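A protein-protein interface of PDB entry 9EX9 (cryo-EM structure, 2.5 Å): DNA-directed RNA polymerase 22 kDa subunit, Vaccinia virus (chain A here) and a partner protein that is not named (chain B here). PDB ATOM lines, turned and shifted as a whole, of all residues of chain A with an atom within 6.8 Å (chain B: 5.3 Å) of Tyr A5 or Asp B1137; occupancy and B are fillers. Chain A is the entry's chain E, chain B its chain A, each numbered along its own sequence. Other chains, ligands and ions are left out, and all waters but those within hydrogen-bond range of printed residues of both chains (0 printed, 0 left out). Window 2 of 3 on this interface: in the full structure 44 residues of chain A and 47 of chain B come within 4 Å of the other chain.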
ATOM      1  N   MET A   2     -29.918 -10.346  12.294  1.00  0.00           N
ATOM      2  CA  MET A   2     -29.180  -9.111  12.107  1.00  0.00           C
ATOM      3  C   MET A   2     -28.434  -8.740  13.384  1.00  0.00           C
ATOM      4  O   MET A   2     -28.059  -9.649  14.163  1.00  0.00           O
ATOM      5  CB  MET A   2     -30.128  -7.990  11.697  1.00  0.00           C
ATOM      6  CG  MET A   2     -29.425  -6.656  11.895  1.00  0.00           C
ATOM      7  SD  MET A   2     -30.487  -5.345  11.240  1.00  0.00           S
ATOM      8  CE  MET A   2     -32.194  -5.954  11.206  1.00  0.00           C
ATOM      9  N   ASN A   3     -27.126  -8.881  13.944  1.00  0.00           N
ATOM     10  CA  ASN A   3     -26.602  -8.301  15.174  1.00  0.00           C
ATOM     11  C   ASN A   3     -25.685  -7.123  14.871  1.00  0.00           C
ATOM     12  O   ASN A   3     -25.720  -6.570  13.779  1.00  0.00           O
ATOM     13  CB  ASN A   3     -25.860  -9.357  15.990  1.00  0.00           C
ATOM     14  CG  ASN A   3     -24.626  -9.870  15.295  1.00  0.00           C
ATOM     15  OD1 ASN A   3     -23.608  -9.186  15.228  1.00  0.00           O
ATOM     16  ND2 ASN A   3     -24.703 -11.088  14.779  1.00  0.00           N
ATOM     17  N   GLN A   4     -24.869  -6.738  15.850  1.00  0.00           N
ATOM     18  CA  GLN A   4     -24.043  -5.546  15.728  1.00  0.00           C
ATOM     19  C   GLN A   4     -22.756  -5.779  14.954  1.00  0.00           C
ATOM     20  O   GLN A   4     -22.030  -4.814  14.699  1.00  0.00           O
ATOM     21  CB  GLN A   4     -23.693  -5.008  17.116  1.00  0.00           C
ATOM     22  CG  GLN A   4     -22.857  -5.963  17.951  1.00  0.00           C
ATOM     23  CD  GLN A   4     -22.442  -5.378  19.281  1.00  0.00           C
ATOM     24  OE1 GLN A   4     -22.573  -6.022  20.320  1.00  0.00           O
ATOM     25  NE2 GLN A   4     -21.928  -4.154  19.258  1.00  0.00           N
ATOM     26  N   TYR A   5     -22.445  -7.018  14.584  1.00  0.00           N
ATOM     27  CA  TYR A   5     -21.197  -7.329  13.904  1.00  0.00           C
ATOM     28  C   TYR A   5     -21.390  -7.665  12.436  1.00  0.00           C
ATOM     29  O   TYR A   5     -20.692  -7.110  11.585  1.00  0.00           O
ATOM     30  CB  TYR A   5     -20.490  -8.491  14.614  1.00  0.00           C
ATOM     31  CG  TYR A   5     -20.042  -8.165  16.019  1.00  0.00           C
ATOM     32  CD1 TYR A   5     -19.576  -6.903  16.346  1.00  0.00           C
ATOM     33  CD2 TYR A   5     -20.092  -9.120  17.022  1.00  0.00           C
ATOM     34  CE1 TYR A   5     -19.171  -6.600  17.627  1.00  0.00           C
ATOM     35  CE2 TYR A   5     -19.687  -8.826  18.306  1.00  0.00           C
ATOM     36  CZ  TYR A   5     -19.229  -7.563  18.602  1.00  0.00           C
ATOM     37  OH  TYR A   5     -18.823  -7.261  19.878  1.00  0.00           O
ATOM     38  N   ASN A   6     -22.326  -8.551  12.103  1.00  0.00           N
ATOM     39  CA  ASN A   6     -22.492  -8.928  10.706  1.00  0.00           C
ATOM     40  C   ASN A   6     -22.957  -7.759   9.847  1.00  0.00           C
ATOM     41  O   ASN A   6     -22.826  -7.817   8.621  1.00  0.00           O
ATOM     42  CB  ASN A   6     -23.461 -10.104  10.582  1.00  0.00           C
ATOM     43  CG  ASN A   6     -24.830  -9.798  11.129  1.00  0.00           C
ATOM     44  OD1 ASN A   6     -25.171  -8.645  11.366  1.00  0.00           O
ATOM     45  ND2 ASN A   6     -25.628 -10.835  11.329  1.00  0.00           N
ATOM     46  N   VAL A   7     -23.485  -6.695  10.450  1.00  0.00           N
ATOM     47  CA  VAL A   7     -23.814  -5.510   9.667  1.00  0.00           C
ATOM     48  C   VAL A   7     -22.545  -4.866   9.126  1.00  0.00           C
ATOM     49  O   VAL A   7     -22.528  -4.338   8.009  1.00  0.00           O
ATOM     50  CB  VAL A   7     -24.644  -4.516  10.497  1.00  0.00           C
ATOM     51  CG1 VAL A   7     -25.991  -5.113  10.836  1.00  0.00           C
ATOM     52  CG2 VAL A   7     -23.903  -4.104  11.758  1.00  0.00           C
ATOM     53  N   LYS A   8     -21.463  -4.900   9.903  1.00  0.00           N
ATOM     54  CA  LYS A   8     -20.199  -4.360   9.419  1.00  0.00           C
ATOM     55  C   LYS A   8     -19.613  -5.213   8.303  1.00  0.00           C
ATOM     56  O   LYS A   8     -18.787  -4.727   7.526  1.00  0.00           O
ATOM     57  CB  LYS A   8     -19.206  -4.238  10.570  1.00  0.00           C
ATOM     58  CG  LYS A   8     -19.647  -3.274  11.656  1.00  0.00           C
ATOM     59  CD  LYS A   8     -18.506  -2.919  12.590  1.00  0.00           C
ATOM     60  CE  LYS A   8     -17.975  -4.139  13.314  1.00  0.00           C
ATOM     61  NZ  LYS A   8     -16.887  -3.783  14.259  1.00  0.00           N
ATOM     62  N   TYR A   9     -20.004  -6.484   8.220  1.00  0.00           N
ATOM     63  CA  TYR A   9     -19.595  -7.318   7.096  1.00  0.00           C
ATOM     64  C   TYR A   9     -20.477  -7.074   5.878  1.00  0.00           C
ATOM     65  O   TYR A   9     -19.997  -7.116   4.742  1.00  0.00           O
ATOM     66  CB  TYR A   9     -19.649  -8.794   7.483  1.00  0.00           C
ATOM     67  CG  TYR A   9     -18.926  -9.151   8.760  1.00  0.00           C
ATOM     68  CD1 TYR A   9     -17.946  -8.329   9.288  1.00  0.00           C
ATOM     69  CD2 TYR A   9     -19.223 -10.323   9.431  1.00  0.00           C
ATOM     70  CE1 TYR A   9     -17.289  -8.664  10.451  1.00  0.00           C
ATOM     71  CE2 TYR A   9     -18.573 -10.661  10.592  1.00  0.00           C
ATOM     72  CZ  TYR A   9     -17.607  -9.832  11.096  1.00  0.00           C
ATOM     73  OH  TYR A   9     -16.962 -10.178  12.253  1.00  0.00           O
ATOM     74  N   LEU A  10     -21.768  -6.828   6.097  1.00  0.00           N
ATOM     75  CA  LEU A  10     -22.686  -6.610   4.985  1.00  0.00           C
ATOM     76  C   LEU A  10     -22.496  -5.240   4.353  1.00  0.00           C
ATOM     77  O   LEU A  10     -22.791  -5.059   3.164  1.00  0.00           O
ATOM     78  CB  LEU A  10     -24.125  -6.773   5.471  1.00  0.00           C
ATOM     79  CG  LEU A  10     -25.249  -6.561   4.460  1.00  0.00           C
ATOM     80  CD1 LEU A  10     -25.191  -7.606   3.379  1.00  0.00           C
ATOM     81  CD2 LEU A  10     -26.589  -6.598   5.157  1.00  0.00           C
ATOM     82  N   TYR A  42     -26.930   1.114  13.802  1.00  0.00           N
ATOM     83  CA  TYR A  42     -27.486  -0.188  14.129  1.00  0.00           C
ATOM     84  C   TYR A  42     -28.723  -0.059  15.004  1.00  0.00           C
ATOM     85  O   TYR A  42     -28.840   0.852  15.827  1.00  0.00           O
ATOM     86  CB  TYR A  42     -26.452  -1.057  14.845  1.00  0.00           C
ATOM     87  CG  TYR A  42     -27.034  -2.361  15.329  1.00  0.00           C
ATOM     88  CD1 TYR A  42     -27.228  -3.419  14.459  1.00  0.00           C
ATOM     89  CD2 TYR A  42     -27.411  -2.528  16.651  1.00  0.00           C
ATOM     90  CE1 TYR A  42     -27.769  -4.609  14.889  1.00  0.00           C
ATOM     91  CE2 TYR A  42     -27.954  -3.716  17.092  1.00  0.00           C
ATOM     92  CZ  TYR A  42     -28.132  -4.751  16.206  1.00  0.00           C
ATOM     93  OH  TYR A  42     -28.671  -5.939  16.638  1.00  0.00           O
ATOM     94  N   LEU A 101     -22.399 -14.466   6.594  1.00  0.00           N
ATOM     95  CA  LEU A 101     -21.950 -13.325   7.382  1.00  0.00           C
ATOM     96  C   LEU A 101     -21.314 -13.736   8.704  1.00  0.00           C
ATOM     97  O   LEU A 101     -21.266 -12.929   9.634  1.00  0.00           O
ATOM     98  CB  LEU A 101     -23.118 -12.374   7.635  1.00  0.00           C
ATOM     99  CG  LEU A 101     -23.940 -12.023   6.397  1.00  0.00           C
ATOM    100  CD1 LEU A 101     -25.086 -11.109   6.755  1.00  0.00           C
ATOM    101  CD2 LEU A 101     -23.065 -11.379   5.353  1.00  0.00           C
ATOM    102  N   LYS B 987      -8.146  -9.215  18.646  1.00  0.00           N
ATOM    103  CA  LYS B 987      -9.212  -9.998  18.039  1.00  0.00           C
ATOM    104  C   LYS B 987      -8.892 -11.483  18.088  1.00  0.00           C
ATOM    105  O   LYS B 987      -9.794 -12.315  18.234  1.00  0.00           O
ATOM    106  CB  LYS B 987      -9.432  -9.544  16.598  1.00  0.00           C
ATOM    107  CG  LYS B 987      -9.866  -8.098  16.471  1.00  0.00           C
ATOM    108  CD  LYS B 987      -9.955  -7.678  15.021  1.00  0.00           C
ATOM    109  CE  LYS B 987     -10.348  -6.222  14.889  1.00  0.00           C
ATOM    110  NZ  LYS B 987     -11.720  -5.975  15.393  1.00  0.00           N
ATOM    111  N   LEU B1133     -18.126 -18.703  15.422  1.00  0.00           N
ATOM    112  CA  LEU B1133     -17.417 -17.448  15.223  1.00  0.00           C
ATOM    113  C   LEU B1133     -18.348 -16.273  14.982  1.00  0.00           C
ATOM    114  O   LEU B1133     -17.881 -15.132  14.959  1.00  0.00           O
ATOM    115  CB  LEU B1133     -16.457 -17.574  14.041  1.00  0.00           C
ATOM    116  CG  LEU B1133     -15.376 -18.646  14.160  1.00  0.00           C
ATOM    117  CD1 LEU B1133     -14.607 -18.771  12.867  1.00  0.00           C
ATOM    118  CD2 LEU B1133     -14.442 -18.318  15.298  1.00  0.00           C
ATOM    119  N   GLY B1134     -19.647 -16.511  14.827  1.00  0.00           N
ATOM    120  CA  GLY B1134     -20.541 -15.476  14.344  1.00  0.00           C
ATOM    121  C   GLY B1134     -20.751 -14.313  15.289  1.00  0.00           C
ATOM    122  O   GLY B1134     -21.422 -13.350  14.907  1.00  0.00           O
ATOM    123  N   SER B1135     -20.201 -14.372  16.501  1.00  0.00           N
ATOM    124  CA  SER B1135     -20.432 -13.353  17.513  1.00  0.00           C
ATOM    125  C   SER B1135     -19.119 -12.939  18.178  1.00  0.00           C
ATOM    126  O   SER B1135     -19.026 -12.815  19.394  1.00  0.00           O
ATOM    127  CB  SER B1135     -21.408 -13.872  18.559  1.00  0.00           C
ATOM    128  OG  SER B1135     -20.893 -15.047  19.154  1.00  0.00           O
ATOM    129  N   PHE B1136     -18.081 -12.703  17.373  1.00  0.00           N
ATOM    130  CA  PHE B1136     -16.761 -12.456  17.939  1.00  0.00           C
ATOM    131  C   PHE B1136     -16.050 -11.236  17.365  1.00  0.00           C
ATOM    132  O   PHE B1136     -14.886 -11.007  17.710  1.00  0.00           O
ATOM    133  CB  PHE B1136     -15.869 -13.682  17.751  1.00  0.00           C
ATOM    134  CG  PHE B1136     -15.900 -14.639  18.901  1.00  0.00           C
ATOM    135  CD1 PHE B1136     -15.162 -14.391  20.040  1.00  0.00           C
ATOM    136  CD2 PHE B1136     -16.651 -15.793  18.840  1.00  0.00           C
ATOM    137  CE1 PHE B1136     -15.183 -15.270  21.095  1.00  0.00           C
ATOM    138  CE2 PHE B1136     -16.670 -16.677  19.896  1.00  0.00           C
ATOM    139  CZ  PHE B1136     -15.936 -16.414  21.021  1.00  0.00           C
ATOM    140  N   ASP B1137     -16.692 -10.437  16.520  1.00  0.00           N
ATOM    141  CA  ASP B1137     -16.089  -9.198  16.029  1.00  0.00           C
ATOM    142  C   ASP B1137     -14.741  -9.472  15.360  1.00  0.00           C
ATOM    143  O   ASP B1137     -13.685  -9.038  15.820  1.00  0.00           O
ATOM    144  CB  ASP B1137     -15.927  -8.196  17.171  1.00  0.00           C
ATOM    145  CG  ASP B1137     -15.316  -6.891  16.717  1.00  0.00           C
ATOM    146  OD1 ASP B1137     -15.173  -6.687  15.496  1.00  0.00           O
ATOM    147  OD2 ASP B1137     -14.972  -6.064  17.583  1.00  0.00           O
ATOM    148  N   LEU B1138     -14.792 -10.221  14.267  1.00  0.00           N
ATOM    149  CA  LEU B1138     -13.597 -10.552  13.497  1.00  0.00           C
ATOM    150  C   LEU B1138     -13.478  -9.654  12.267  1.00  0.00           C
ATOM    151  O   LEU B1138     -13.352 -10.115  11.137  1.00  0.00           O
ATOM    152  CB  LEU B1138     -13.629 -12.021  13.101  1.00  0.00           C
ATOM    153  CG  LEU B1138     -13.708 -12.986  14.274  1.00  0.00           C
ATOM    154  CD1 LEU B1138     -14.084 -14.364  13.792  1.00  0.00           C
ATOM    155  CD2 LEU B1138     -12.382 -13.016  14.992  1.00  0.00           C
ATOM    156  N   GLU B1139     -13.499  -8.348  12.500  1.00  0.00           N
ATOM    157  CA  GLU B1139     -13.426  -7.395  11.404  1.00  0.00           C
ATOM    158  C   GLU B1139     -11.985  -7.203  10.958  1.00  0.00           C
ATOM    159  O   GLU B1139     -11.079  -7.050  11.781  1.00  0.00           O
ATOM    160  CB  GLU B1139     -14.019  -6.053  11.818  1.00  0.00           C
ATOM    161  CG  GLU B1139     -14.269  -5.135  10.648  1.00  0.00           C
ATOM    162  CD  GLU B1139     -14.657  -3.739  11.068  1.00  0.00           C
ATOM    163  OE1 GLU B1139     -14.440  -3.387  12.245  1.00  0.00           O
ATOM    164  OE2 GLU B1139     -15.179  -2.988  10.219  1.00  0.00           O
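Among the printed residues, merely in contact across the chains: Tyr A5 with Asp B1137 (3.6 Å), Tyr A9 with Asp B1137 (3.9 Å), Tyr A9 with Glu B1139 (3.9 Å) and Asn A3 with Gly B1134 (3.99 Å).
Of the printed residues of chain B, Tyr A5 touches Asp B1137. Asp B1137 touches just these residues of chain A: Tyr A5, Lys A8 and Tyr A9. Of the printed residues of chain B, Tyr A9 touches Asp B1137 (3.9 Å), Leu B1138 (3.0 Å) and Glu B1139 (3.9 Å). Printed residues of chain A within 4 Å of Gly B1134: Asn A3 (3.99 Å). Of the printed residues of chain B, Lys A8 touches Asp B1137 and Glu B1139. Of the printed residues of chain A, Glu B1139 touches Lys A8 and Tyr A9. Of the printed residues of chain B, Asn A3 touches Gly B1134. Leu A101 touches none of the printed residues of chain B. The nearest printed residue of chain B that does not touch Asn A3 is Ser B1135 (5.6 Å).
The side-chain amide oxygen of Asn A3 lies within hydrogen-bond range of the backbone NH of Tyr A5 (2.5 Å). The side-chain amino group (NZ) of Lys B987 lies within salt-bridge range of the side-chain carboxylate (OD1) of Asp B1137, 3.5 Å away. The backbone carbonyl oxygen (O) of Asn A3 lies close to the side-chain amide oxygen (OD1) of Asn A6, at 3.2 Å.
The side-chain hydroxyl of Tyr A9 sits at hydrogen-bond distance from the backbone NH of Leu B1138 (3.0 Å). OD1 of Asp B1137 is in salt-bridge range of NZ of Lys A8 (3.6 Å). NZ of Lys A8 is in salt-bridge range of OE1 of Glu B1139, at 3.2 Å.
Of the 8 printed residues of chain B, 4 touch a printed residue of chain A. Hydrophobic or aromatic side chains of chain B within 4 Å of the printed part of chain A: Leu B1138. Of the 11 printed residues of chain A, 4 touch a printed residue of chain B. Among the printed residues, Asp or Glu carboxylates within 4 Å of a Lys or Arg side-chain nitrogen of the other chain: Lys A8 with Asp B1137 (3.6 Å) and Lys A8 with Glu B1139 (3.2 Å).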
